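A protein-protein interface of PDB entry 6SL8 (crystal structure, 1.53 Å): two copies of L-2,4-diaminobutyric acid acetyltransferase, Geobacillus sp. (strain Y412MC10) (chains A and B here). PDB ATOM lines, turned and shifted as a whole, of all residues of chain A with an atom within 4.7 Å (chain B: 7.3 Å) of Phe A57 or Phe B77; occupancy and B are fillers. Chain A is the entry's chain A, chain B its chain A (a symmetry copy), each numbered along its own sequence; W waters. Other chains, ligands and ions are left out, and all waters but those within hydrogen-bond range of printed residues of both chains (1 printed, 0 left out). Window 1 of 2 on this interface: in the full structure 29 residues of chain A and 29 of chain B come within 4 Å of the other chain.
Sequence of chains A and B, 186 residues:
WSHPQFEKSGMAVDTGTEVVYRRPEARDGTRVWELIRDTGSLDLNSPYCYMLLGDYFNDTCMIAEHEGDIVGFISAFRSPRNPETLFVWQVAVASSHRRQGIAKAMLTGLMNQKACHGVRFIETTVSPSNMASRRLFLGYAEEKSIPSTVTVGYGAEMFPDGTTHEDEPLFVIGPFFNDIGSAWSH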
ATOM      1  N   LEU A  52       4.969 -37.229 -25.473  1.00  0.00           N
ATOM      2  CA  LEU A  52       5.201 -35.992 -24.744  1.00  0.00           C
ATOM      3  C   LEU A  52       5.270 -36.145 -23.244  1.00  0.00           C
ATOM      4  O   LEU A  52       6.092 -35.525 -22.526  1.00  0.00           O
ATOM      5  CB  LEU A  52       4.134 -34.926 -25.055  1.00  0.00           C
ATOM      6  CG  LEU A  52       4.095 -34.179 -26.289  1.00  0.00           C
ATOM      7  CD1 LEU A  52       3.052 -33.050 -26.062  1.00  0.00           C
ATOM      8  CD2 LEU A  52       5.446 -33.575 -26.682  1.00  0.00           C
ATOM      9  N   LEU A  53       4.339 -36.931 -22.692  1.00  0.00           N
ATOM     10  CA  LEU A  53       4.342 -37.222 -21.271  1.00  0.00           C
ATOM     11  C   LEU A  53       5.600 -37.848 -20.831  1.00  0.00           C
ATOM     12  O   LEU A  53       6.211 -37.408 -19.871  1.00  0.00           O
ATOM     13  CB  LEU A  53       3.116 -38.006 -20.839  1.00  0.00           C
ATOM     14  CG  LEU A  53       1.776 -37.282 -20.968  1.00  0.00           C
ATOM     15  CD1 LEU A  53       0.611 -38.254 -20.812  1.00  0.00           C
ATOM     16  CD2 LEU A  53       1.689 -36.261 -19.842  1.00  0.00           C
ATOM     17  N   ASP A  55       8.541 -37.578 -22.380  1.00  0.00           N
ATOM     18  CA  ASP A  55       9.679 -36.697 -22.680  1.00  0.00           C
ATOM     19  C   ASP A  55       9.710 -35.536 -21.674  1.00  0.00           C
ATOM     20  O   ASP A  55      10.758 -35.213 -21.132  1.00  0.00           O
ATOM     21  CB  ASP A  55       9.482 -36.162 -24.062  1.00  0.00           C
ATOM     22  CG  ASP A  55      10.771 -35.771 -24.776  1.00  0.00           C
ATOM     23  OD1 ASP A  55      11.822 -35.888 -24.163  1.00  0.00           O
ATOM     24  OD2 ASP A  55      10.702 -35.517 -25.991  1.00  0.00           O
ATOM     25  N   TYR A  56       8.553 -34.872 -21.439  1.00  0.00           N
ATOM     26  CA  TYR A  56       8.519 -33.666 -20.643  1.00  0.00           C
ATOM     27  C   TYR A  56       7.972 -33.778 -19.218  1.00  0.00           C
ATOM     28  O   TYR A  56       8.276 -32.933 -18.351  1.00  0.00           O
ATOM     29  CB  TYR A  56       7.723 -32.563 -21.395  1.00  0.00           C
ATOM     30  CG  TYR A  56       8.410 -32.098 -22.699  1.00  0.00           C
ATOM     31  CD1 TYR A  56       9.423 -31.153 -22.662  1.00  0.00           C
ATOM     32  CD2 TYR A  56       8.150 -32.715 -23.891  1.00  0.00           C
ATOM     33  CE1 TYR A  56      10.073 -30.761 -23.789  1.00  0.00           C
ATOM     34  CE2 TYR A  56       8.780 -32.325 -25.056  1.00  0.00           C
ATOM     35  CZ  TYR A  56       9.815 -31.416 -24.964  1.00  0.00           C
ATOM     36  OH  TYR A  56      10.421 -31.097 -26.170  1.00  0.00           O
ATOM     37  N   PHE A  57       7.076 -34.726 -19.019  1.00  0.00           N
ATOM     38  CA  PHE A  57       6.389 -34.885 -17.712  1.00  0.00           C
ATOM     39  C   PHE A  57       6.775 -36.118 -16.976  1.00  0.00           C
ATOM     40  O   PHE A  57       6.098 -36.601 -16.055  1.00  0.00           O
ATOM     41  CB  PHE A  57       4.850 -34.835 -17.906  1.00  0.00           C
ATOM     42  CG  PHE A  57       4.360 -33.554 -18.416  1.00  0.00           C
ATOM     43  CD1 PHE A  57       4.234 -33.233 -19.776  1.00  0.00           C
ATOM     44  CD2 PHE A  57       4.002 -32.602 -17.487  1.00  0.00           C
ATOM     45  CE1 PHE A  57       3.807 -31.996 -20.212  1.00  0.00           C
ATOM     46  CE2 PHE A  57       3.544 -31.349 -17.902  1.00  0.00           C
ATOM     47  CZ  PHE A  57       3.418 -31.050 -19.250  1.00  0.00           C
ATOM     48  N   ASN A  58       7.981 -36.681 -17.263  1.00  0.00           N
ATOM     49  CA  ASN A  58       8.326 -37.953 -16.724  1.00  0.00           C
ATOM     50  C   ASN A  58       8.569 -37.941 -15.229  1.00  0.00           C
ATOM     51  O   ASN A  58       8.415 -38.986 -14.609  1.00  0.00           O
ATOM     52  CB  ASN A  58       9.449 -38.574 -17.575  1.00  0.00           C
ATOM     53  CG  ASN A  58      10.846 -38.428 -17.032  1.00  0.00           C
ATOM     54  OD1 ASN A  58      11.668 -39.343 -17.265  1.00  0.00           O
ATOM     55  ND2 ASN A  58      11.183 -37.334 -16.489  1.00  0.00           N
ATOM     56  N   ASP A  59       8.845 -36.762 -14.628  1.00  0.00           N
ATOM     57  CA  ASP A  59       8.993 -36.697 -13.196  1.00  0.00           C
ATOM     58  C   ASP A  59       7.687 -36.915 -12.389  1.00  0.00           C
ATOM     59  O   ASP A  59       7.669 -37.148 -11.184  1.00  0.00           O
ATOM     60  CB  ASP A  59       9.587 -35.390 -12.781  1.00  0.00           C
ATOM     61  CG  ASP A  59      11.004 -35.168 -13.317  1.00  0.00           C
ATOM     62  OD1 ASP A  59      11.781 -36.099 -13.128  1.00  0.00           O
ATOM     63  OD2 ASP A  59      11.207 -34.118 -13.987  1.00  0.00           O
ATOM     64  N   THR A  60       6.559 -36.760 -13.109  1.00  0.00           N
ATOM     65  CA  THR A  60       5.269 -36.942 -12.477  1.00  0.00           C
ATOM     66  C   THR A  60       4.462 -38.013 -13.179  1.00  0.00           C
ATOM     67  O   THR A  60       3.187 -38.051 -13.078  1.00  0.00           O
ATOM     68  CB  THR A  60       4.441 -35.617 -12.512  1.00  0.00           C
ATOM     69  OG1 THR A  60       4.460 -35.099 -13.832  1.00  0.00           O
ATOM     70  CG2 THR A  60       5.018 -34.627 -11.503  1.00  0.00           C
ATOM     71  N   CYS A  61       5.088 -38.926 -13.872  1.00  0.00           N
ATOM     72  CA  CYS A  61       4.435 -40.101 -14.414  1.00  0.00           C
ATOM     73  C   CYS A  61       5.168 -41.407 -13.989  1.00  0.00           C
ATOM     74  O   CYS A  61       6.304 -41.370 -13.536  1.00  0.00           O
ATOM     75  CB  CYS A  61       4.375 -40.064 -15.942  1.00  0.00           C
ATOM     76  SG  CYS A  61       3.504 -38.671 -16.672  1.00  0.00           S
ATOM     77  N   ALA A  76       0.461 -37.712 -14.640  1.00  0.00           N
ATOM     78  CA  ALA A  76       0.127 -36.617 -13.724  1.00  0.00           C
ATOM     79  C   ALA A  76       1.048 -35.454 -14.029  1.00  0.00           C
ATOM     80  O   ALA A  76       2.029 -35.575 -14.819  1.00  0.00           O
ATOM     81  CB  ALA A  76       0.311 -37.056 -12.234  1.00  0.00           C
ATOM     82  N   PHE A  77       0.717 -34.289 -13.474  1.00  0.00           N
ATOM     83  CA  PHE A  77       1.547 -33.079 -13.632  1.00  0.00           C
ATOM     84  C   PHE A  77       1.365 -32.216 -12.415  1.00  0.00           C
ATOM     85  O   PHE A  77       0.297 -32.239 -11.810  1.00  0.00           O
ATOM     86  CB  PHE A  77       1.228 -32.279 -14.938  1.00  0.00           C
ATOM     87  CG  PHE A  77      -0.244 -31.986 -15.136  1.00  0.00           C
ATOM     88  CD1 PHE A  77      -0.766 -30.880 -14.562  1.00  0.00           C
ATOM     89  CD2 PHE A  77      -1.037 -32.839 -15.935  1.00  0.00           C
ATOM     90  CE1 PHE A  77      -2.121 -30.571 -14.727  1.00  0.00           C
ATOM     91  CE2 PHE A  77      -2.446 -32.544 -16.093  1.00  0.00           C
ATOM     92  CZ  PHE A  77      -2.929 -31.413 -15.488  1.00  0.00           C
ATOM     93  N   LEU B  53      -6.350 -28.696 -20.660  1.00  0.00           N
ATOM     94  CA  LEU B  53      -5.547 -27.589 -21.142  1.00  0.00           C
ATOM     95  C   LEU B  53      -6.131 -26.283 -20.798  1.00  0.00           C
ATOM     96  O   LEU B  53      -5.455 -25.421 -20.261  1.00  0.00           O
ATOM     97  CB  LEU B  53      -5.219 -27.713 -22.620  1.00  0.00           C
ATOM     98  CG  LEU B  53      -4.328 -28.891 -23.013  1.00  0.00           C
ATOM     99  CD1 LEU B  53      -4.327 -29.097 -24.524  1.00  0.00           C
ATOM    100  CD2 LEU B  53      -2.904 -28.562 -22.584  1.00  0.00           C
ATOM    101  N   PHE B  57      -3.615 -25.367 -17.964  1.00  0.00           N
ATOM    102  CA  PHE B  57      -2.528 -24.805 -18.806  1.00  0.00           C
ATOM    103  C   PHE B  57      -2.917 -23.574 -19.545  1.00  0.00           C
ATOM    104  O   PHE B  57      -2.296 -23.148 -20.531  1.00  0.00           O
ATOM    105  CB  PHE B  57      -2.005 -25.881 -19.794  1.00  0.00           C
ATOM    106  CG  PHE B  57      -1.389 -27.036 -19.139  1.00  0.00           C
ATOM    107  CD1 PHE B  57      -2.083 -28.186 -18.732  1.00  0.00           C
ATOM    108  CD2 PHE B  57      -0.033 -26.978 -18.906  1.00  0.00           C
ATOM    109  CE1 PHE B  57      -1.469 -29.233 -18.078  1.00  0.00           C
ATOM    110  CE2 PHE B  57       0.618 -28.036 -18.266  1.00  0.00           C
ATOM    111  CZ  PHE B  57      -0.081 -29.169 -17.878  1.00  0.00           C
ATOM    112  N   THR B  60      -0.548 -20.755 -20.907  1.00  0.00           N
ATOM    113  CA  THR B  60       0.304 -21.016 -22.048  1.00  0.00           C
ATOM    114  C   THR B  60      -0.491 -21.565 -23.212  1.00  0.00           C
ATOM    115  O   THR B  60       0.075 -22.244 -24.137  1.00  0.00           O
ATOM    116  CB  THR B  60       1.412 -22.059 -21.689  1.00  0.00           C
ATOM    117  OG1 THR B  60       0.805 -23.172 -21.053  1.00  0.00           O
ATOM    118  CG2 THR B  60       2.464 -21.400 -20.800  1.00  0.00           C
ATOM    119  N   CYS B  61      -1.771 -21.314 -23.279  1.00  0.00           N
ATOM    120  CA  CYS B  61      -2.582 -21.619 -24.442  1.00  0.00           C
ATOM    121  C   CYS B  61      -3.371 -20.369 -24.930  1.00  0.00           C
ATOM    122  O   CYS B  61      -3.499 -19.387 -24.212  1.00  0.00           O
ATOM    123  CB  CYS B  61      -3.588 -22.735 -24.155  1.00  0.00           C
ATOM    124  SG  CYS B  61      -2.903 -24.315 -23.640  1.00  0.00           S
ATOM    125  N   SER B  75      -1.927 -24.797 -28.186  1.00  0.00           N
ATOM    126  CA  SER B  75      -1.604 -25.410 -26.923  1.00  0.00           C
ATOM    127  C   SER B  75      -0.110 -25.388 -26.717  1.00  0.00           C
ATOM    128  O   SER B  75       0.672 -25.667 -27.621  1.00  0.00           O
ATOM    129  CB  SER B  75      -2.141 -26.797 -26.738  1.00  0.00           C
ATOM    130  OG  SER B  75      -1.713 -27.646 -27.808  1.00  0.00           O
ATOM    131  N   ALA B  76       0.313 -25.099 -25.471  1.00  0.00           N
ATOM    132  CA  ALA B  76       1.736 -25.093 -25.119  1.00  0.00           C
ATOM    133  C   ALA B  76       1.847 -25.213 -23.613  1.00  0.00           C
ATOM    134  O   ALA B  76       0.830 -25.128 -22.866  1.00  0.00           O
ATOM    135  CB  ALA B  76       2.425 -23.771 -25.594  1.00  0.00           C
ATOM    136  N   PHE B  77       3.062 -25.483 -23.140  1.00  0.00           N
ATOM    137  CA  PHE B  77       3.340 -25.574 -21.694  1.00  0.00           C
ATOM    138  C   PHE B  77       4.769 -25.175 -21.458  1.00  0.00           C
ATOM    139  O   PHE B  77       5.608 -25.384 -22.330  1.00  0.00           O
ATOM    140  CB  PHE B  77       3.048 -26.990 -21.097  1.00  0.00           C
ATOM    141  CG  PHE B  77       3.688 -28.125 -21.868  1.00  0.00           C
ATOM    142  CD1 PHE B  77       4.958 -28.475 -21.572  1.00  0.00           C
ATOM    143  CD2 PHE B  77       2.949 -28.821 -22.851  1.00  0.00           C
ATOM    144  CE1 PHE B  77       5.582 -29.523 -22.258  1.00  0.00           C
ATOM    145  CE2 PHE B  77       3.592 -29.891 -23.586  1.00  0.00           C
ATOM    146  CZ  PHE B  77       4.883 -30.205 -23.250  1.00  0.00           C
ATOM    147  N   ARG B  78       5.057 -24.686 -20.293  1.00  0.00           N
ATOM    148  CA  ARG B  78       6.464 -24.537 -19.895  1.00  0.00           C
ATOM    149  C   ARG B  78       6.955 -25.940 -19.480  1.00  0.00           C
ATOM    150  O   ARG B  78       6.306 -26.693 -18.745  1.00  0.00           O
ATOM    151  CB  ARG B  78       6.630 -23.572 -18.699  1.00  0.00           C
ATOM    152  CG  ARG B  78       6.206 -22.145 -19.002  1.00  0.00           C
ATOM    153  CD  ARG B  78       6.943 -21.565 -20.196  1.00  0.00           C
ATOM    154  NE  ARG B  78       6.676 -20.113 -20.341  1.00  0.00           N
ATOM    155  CZ  ARG B  78       7.483 -19.123 -19.890  1.00  0.00           C
ATOM    156  NH1 ARG B  78       7.040 -17.869 -20.046  1.00  0.00           N
ATOM    157  NH2 ARG B  78       8.629 -19.346 -19.321  1.00  0.00           N
ATOM    158  N   SER B  79       8.158 -26.313 -19.952  1.00  0.00           N
ATOM    159  CA  SER B  79       8.690 -27.600 -19.595  1.00  0.00           C
ATOM    160  C   SER B  79       8.944 -27.724 -18.096  1.00  0.00           C
ATOM    161  O   SER B  79       9.564 -26.835 -17.516  1.00  0.00           O
ATOM    162  CB  SER B  79      10.023 -27.780 -20.348  1.00  0.00           C
ATOM    163  OG  SER B  79      10.688 -28.927 -19.858  1.00  0.00           O
ATOM    164  N   PRO B  80       8.391 -28.767 -17.441  1.00  0.00           N
ATOM    165  CA  PRO B  80       8.572 -28.831 -15.982  1.00  0.00           C
ATOM    166  C   PRO B  80      10.048 -28.782 -15.541  1.00  0.00           C
ATOM    167  O   PRO B  80      10.318 -28.131 -14.558  1.00  0.00           O
ATOM    168  CB  PRO B  80       7.944 -30.198 -15.630  1.00  0.00           C
ATOM    169  CG  PRO B  80       6.832 -30.305 -16.618  1.00  0.00           C
ATOM    170  CD  PRO B  80       7.392 -29.743 -17.926  1.00  0.00           C
ATOM    171  N   ARG B  81      10.925 -29.425 -16.260  1.00  0.00           N
ATOM    172  CA  ARG B  81      12.380 -29.429 -15.936  1.00  0.00           C
ATOM    173  C   ARG B  81      13.085 -28.121 -16.227  1.00  0.00           C
ATOM    174  O   ARG B  81      14.164 -27.793 -15.607  1.00  0.00           O
ATOM    175  CB  ARG B  81      13.116 -30.467 -16.763  1.00  0.00           C
ATOM    176  CG  ARG B  81      12.995 -31.896 -16.297  1.00  0.00           C
ATOM    177  CD  ARG B  81      14.201 -32.668 -16.838  1.00  0.00           C
ATOM    178  NE  ARG B  81      14.621 -32.193 -18.180  1.00  0.00           N
ATOM    179  CZ  ARG B  81      15.878 -32.198 -18.621  1.00  0.00           C
ATOM    180  NH1 ARG B  81      16.152 -31.762 -19.836  1.00  0.00           N
ATOM    181  NH2 ARG B  81      16.850 -32.645 -17.845  1.00  0.00           N
ATOM    182  N   ASN B  82      12.564 -27.388 -17.206  1.00  0.00           N
ATOM    183  CA  ASN B  82      13.270 -26.230 -17.819  1.00  0.00           C
ATOM    184  C   ASN B  82      12.239 -25.159 -18.066  1.00  0.00           C
ATOM    185  O   ASN B  82      11.737 -24.979 -19.196  1.00  0.00           O
ATOM    186  CB  ASN B  82      13.905 -26.664 -19.146  1.00  0.00           C
ATOM    187  CG  ASN B  82      15.046 -27.657 -18.990  1.00  0.00           C
ATOM    188  OD1 ASN B  82      16.067 -27.336 -18.406  1.00  0.00           O
ATOM    189  ND2 ASN B  82      14.920 -28.825 -19.569  1.00  0.00           N
ATOM    190  N   PRO B  83      11.874 -24.408 -17.024  1.00  0.00           N
ATOM    191  CA  PRO B  83      10.754 -23.469 -17.121  1.00  0.00           C
ATOM    192  C   PRO B  83      10.927 -22.353 -18.119  1.00  0.00           C
ATOM    193  O   PRO B  83       9.964 -21.765 -18.526  1.00  0.00           O
ATOM    194  CB  PRO B  83      10.643 -22.866 -15.690  1.00  0.00           C
ATOM    195  CG  PRO B  83      11.755 -23.413 -14.901  1.00  0.00           C
ATOM    196  CD  PRO B  83      12.455 -24.454 -15.663  1.00  0.00           C
ATOM    197  N   THR B  85      11.779 -22.959 -21.125  1.00  0.00           N
ATOM    198  CA  THR B  85      11.444 -23.504 -22.419  1.00  0.00           C
ATOM    199  C   THR B  85       9.916 -23.647 -22.554  1.00  0.00           C
ATOM    200  O   THR B  85       9.283 -24.219 -21.619  1.00  0.00           O
ATOM    201  CB  THR B  85      12.085 -24.894 -22.588  1.00  0.00           C
ATOM    202  OG1 THR B  85      13.525 -24.719 -22.645  1.00  0.00           O
ATOM    203  CG2 THR B  85      11.618 -25.589 -23.801  1.00  0.00           C
ATOM    204  N   LEU B  86       9.380 -23.048 -23.576  1.00  0.00           N
ATOM    205  CA  LEU B  86       8.007 -23.133 -23.959  1.00  0.00           C
ATOM    206  C   LEU B  86       7.923 -24.257 -25.025  1.00  0.00           C
ATOM    207  O   LEU B  86       8.440 -24.059 -26.105  1.00  0.00           O
ATOM    208  CB  LEU B  86       7.446 -21.813 -24.472  1.00  0.00           C
ATOM    209  CG  LEU B  86       5.955 -21.784 -24.871  1.00  0.00           C
ATOM    210  CD1 LEU B  86       5.050 -21.872 -23.626  1.00  0.00           C
ATOM    211  CD2 LEU B  86       5.679 -20.600 -25.773  1.00  0.00           C
ATOM    212  N   PHE B  87       7.202 -25.337 -24.710  1.00  0.00           N
ATOM    213  CA  PHE B  87       6.896 -26.381 -25.732  1.00  0.00           C
ATOM    214  C   PHE B  87       5.584 -26.078 -26.348  1.00  0.00           C
ATOM    215  O   PHE B  87       4.558 -26.049 -25.623  1.00  0.00           O
ATOM    216  CB  PHE B  87       6.933 -27.766 -25.110  1.00  0.00           C
ATOM    217  CG  PHE B  87       6.749 -28.839 -26.176  1.00  0.00           C
ATOM    218  CD1 PHE B  87       7.843 -29.278 -26.828  1.00  0.00           C
ATOM    219  CD2 PHE B  87       5.496 -29.276 -26.580  1.00  0.00           C
ATOM    220  CE1 PHE B  87       7.747 -30.203 -27.885  1.00  0.00           C
ATOM    221  CE2 PHE B  87       5.390 -30.219 -27.631  1.00  0.00           C
ATOM    222  CZ  PHE B  87       6.518 -30.634 -28.241  1.00  0.00           C
ATOM    223  N   VAL B  88       5.542 -25.888 -27.663  1.00  0.00           N
ATOM    224  CA  VAL B  88       4.356 -25.650 -28.421  1.00  0.00           C
ATOM    225  C   VAL B  88       3.871 -26.962 -28.956  1.00  0.00           C
ATOM    226  O   VAL B  88       4.570 -27.643 -29.757  1.00  0.00           O
ATOM    227  CB  VAL B  88       4.458 -24.547 -29.488  1.00  0.00           C
ATOM    228  CG1 VAL B  88       3.179 -24.436 -30.251  1.00  0.00           C
ATOM    229  CG2 VAL B  88       4.882 -23.227 -28.838  1.00  0.00           C
ATOM    230  N   TRP B  89       2.649 -27.377 -28.566  1.00  0.00           N
ATOM    231  CA  TRP B  89       2.136 -28.700 -28.819  1.00  0.00           C
ATOM    232  C   TRP B  89       1.309 -28.686 -30.105  1.00  0.00           C
ATOM    233  O   TRP B  89       1.700 -29.397 -31.061  1.00  0.00           O
ATOM    234  CB  TRP B  89       1.348 -29.198 -27.619  1.00  0.00           C
ATOM    235  CG  TRP B  89       0.799 -30.561 -27.664  1.00  0.00           C
ATOM    236  CD1 TRP B  89       0.866 -31.446 -28.722  1.00  0.00           C
ATOM    237  CD2 TRP B  89       0.071 -31.214 -26.629  1.00  0.00           C
ATOM    238  NE1 TRP B  89       0.178 -32.575 -28.385  1.00  0.00           N
ATOM    239  CE2 TRP B  89      -0.280 -32.486 -27.080  1.00  0.00           C
ATOM    240  CE3 TRP B  89      -0.306 -30.810 -25.327  1.00  0.00           C
ATOM    241  CZ2 TRP B  89      -1.050 -33.379 -26.277  1.00  0.00           C
ATOM    242  CZ3 TRP B  89      -1.056 -31.695 -24.517  1.00  0.00           C
ATOM    243  CH2 TRP B  89      -1.366 -32.958 -24.994  1.00  0.00           C
ATOM    244  N   LEU B 110       1.501 -15.822 -26.763  1.00  0.00           N
ATOM    245  CA  LEU B 110       2.180 -16.636 -25.765  1.00  0.00           C
ATOM    246  C   LEU B 110       3.527 -16.114 -25.352  1.00  0.00           C
ATOM    247  O   LEU B 110       4.000 -16.433 -24.290  1.00  0.00           O
ATOM    248  CB  LEU B 110       2.418 -18.079 -26.366  1.00  0.00           C
ATOM    249  CG  LEU B 110       1.170 -18.817 -26.711  1.00  0.00           C
ATOM    250  CD1 LEU B 110       1.609 -20.193 -27.219  1.00  0.00           C
ATOM    251  CD2 LEU B 110       0.273 -18.951 -25.518  1.00  0.00           C
ATOM    252  N   GLU B 123      10.384 -24.901 -28.114  1.00  0.00           N
ATOM    253  CA  GLU B 123      10.544 -26.226 -28.702  1.00  0.00           C
ATOM    254  C   GLU B 123       9.216 -26.656 -29.275  1.00  0.00           C
ATOM    255  O   GLU B 123       8.202 -26.428 -28.667  1.00  0.00           O
ATOM    256  CB  GLU B 123      11.005 -27.208 -27.711  1.00  0.00           C
ATOM    257  CG  GLU B 123      12.441 -27.084 -27.249  1.00  0.00           C
ATOM    258  CD  GLU B 123      12.980 -28.123 -26.330  1.00  0.00           C
ATOM    259  OE1 GLU B 123      14.182 -28.006 -25.975  1.00  0.00           O
ATOM    260  OE2 GLU B 123      12.306 -29.128 -25.930  1.00  0.00           O
HETATM  261  O   HOH W   1      10.449 -31.276 -18.459  1.00  0.00           O
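The side-chain carboxylate (OE2) of Glu B123 is in hydrogen-bond range of the side-chain hydroxyl (OH) of Tyr A56 (2.7 Å).
The backbone NH of Glu B123 lies within hydrogen-bond range of the backbone carbonyl oxygen of Leu B86 (2.9 Å).
The backbone carbonyl oxygen (O) of Phe B77 is in hydrogen-bond range of the backbone NH (N) of Phe B87 (2.9 Å).
O of Phe B57 sits at hydrogen-bond distance from SG of Cys B61, at 3.4 Å.
The backbone carbonyl oxygen (O) of Glu B123 lies within hydrogen-bond range of the backbone NH (N) of Val B88 (2.9 Å).
N of Ser B79 lies within hydrogen-bond range of O of Thr B85 (2.9 Å).
O of Phe B57 is in hydrogen-bond range of OG1 of Thr B60 (3.1 Å).
CD2 of Leu A52 touches CE2 of Phe B87, at 3.5 Å.
Trp B89 touches Leu A52.
Phe B77 touches Tyr A56 (CE1 to CB, 3.8 Å).
Tyr A56 touches Ser B79.
CD of Pro B80 touches O of Tyr A56 (3.3 Å).
Phe B87 touches Tyr A56 (CD1 to OH, 3.2 Å).
CE1 of Phe A57 touches CE1 of Phe B77 (3.7 Å).
CG of Pro B80 touches CE2 of Phe A57, at 3.7 Å.
OD2 of Asp A59 touches CG of Arg B81, 3.7 Å away.
CE1 of Phe A77 touches CE1 of Phe B57, at 3.7 Å.
Phe A57 touches just these residues of chain B: Phe B77 (3.7 Å) and Pro B80 (3.7 Å).
Thr B60 touches none of the printed residues of chain A.
Cys B61 touches none of the printed residues of chain A.
Of chain A, only Tyr A56 and Phe A57 come within 4 Å of Phe B77.
Of the printed residues of chain A, Arg B81 touches Asp A59.
Printed residues of chain A within 4 Å of Phe B87: Leu A52 (3.5 Å) and Tyr A56 (3.2 Å).
Of the printed residues of chain A, Glu B123 touches Tyr A56.
The nearest residue of chain B that does not touch Phe A57 is Phe B57 (4.2 Å).
The nearest residue of chain A that does not touch Phe B77 is Leu A52 (4.05 Å).
Of the 20 printed residues of chain B, 8 touch a printed residue of chain A.
Hydrophobic or aromatic side chains of chain B that line the printed part of chain A: Phe B57, Phe B77, Pro B80, Phe B87 and Trp B89.
Of the 11 printed residues of chain A, 5 touch a printed residue of chain B.
Hydrophobic or aromatic side chains of chain A that line the printed part of chain B: Leu A52, Tyr A56, Phe A57 and Phe A77.
Among the printed residues, 11 pairs touch across the chains.
Among the printed residues, no Asp or Glu carboxylate lies within 4 Å of a Lys or Arg side-chain nitrogen of the other chain.
Phe A57 touches Phe B77, and with the chains exchanged Phe A77 touches Phe B57.
Of the 11 pairs that touch across the chains among the printed residues, 2 have their exchanged pair printed and touching as well.
Water W1 lies within hydrogen-bond range of the backbone carbonyl oxygen (O) of Tyr A56 (2.7 Å), the side-chain hydroxyl (OG) of Ser B79 (2.7 Å) and the backbone NH (N) of Arg B81 (2.9 Å).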
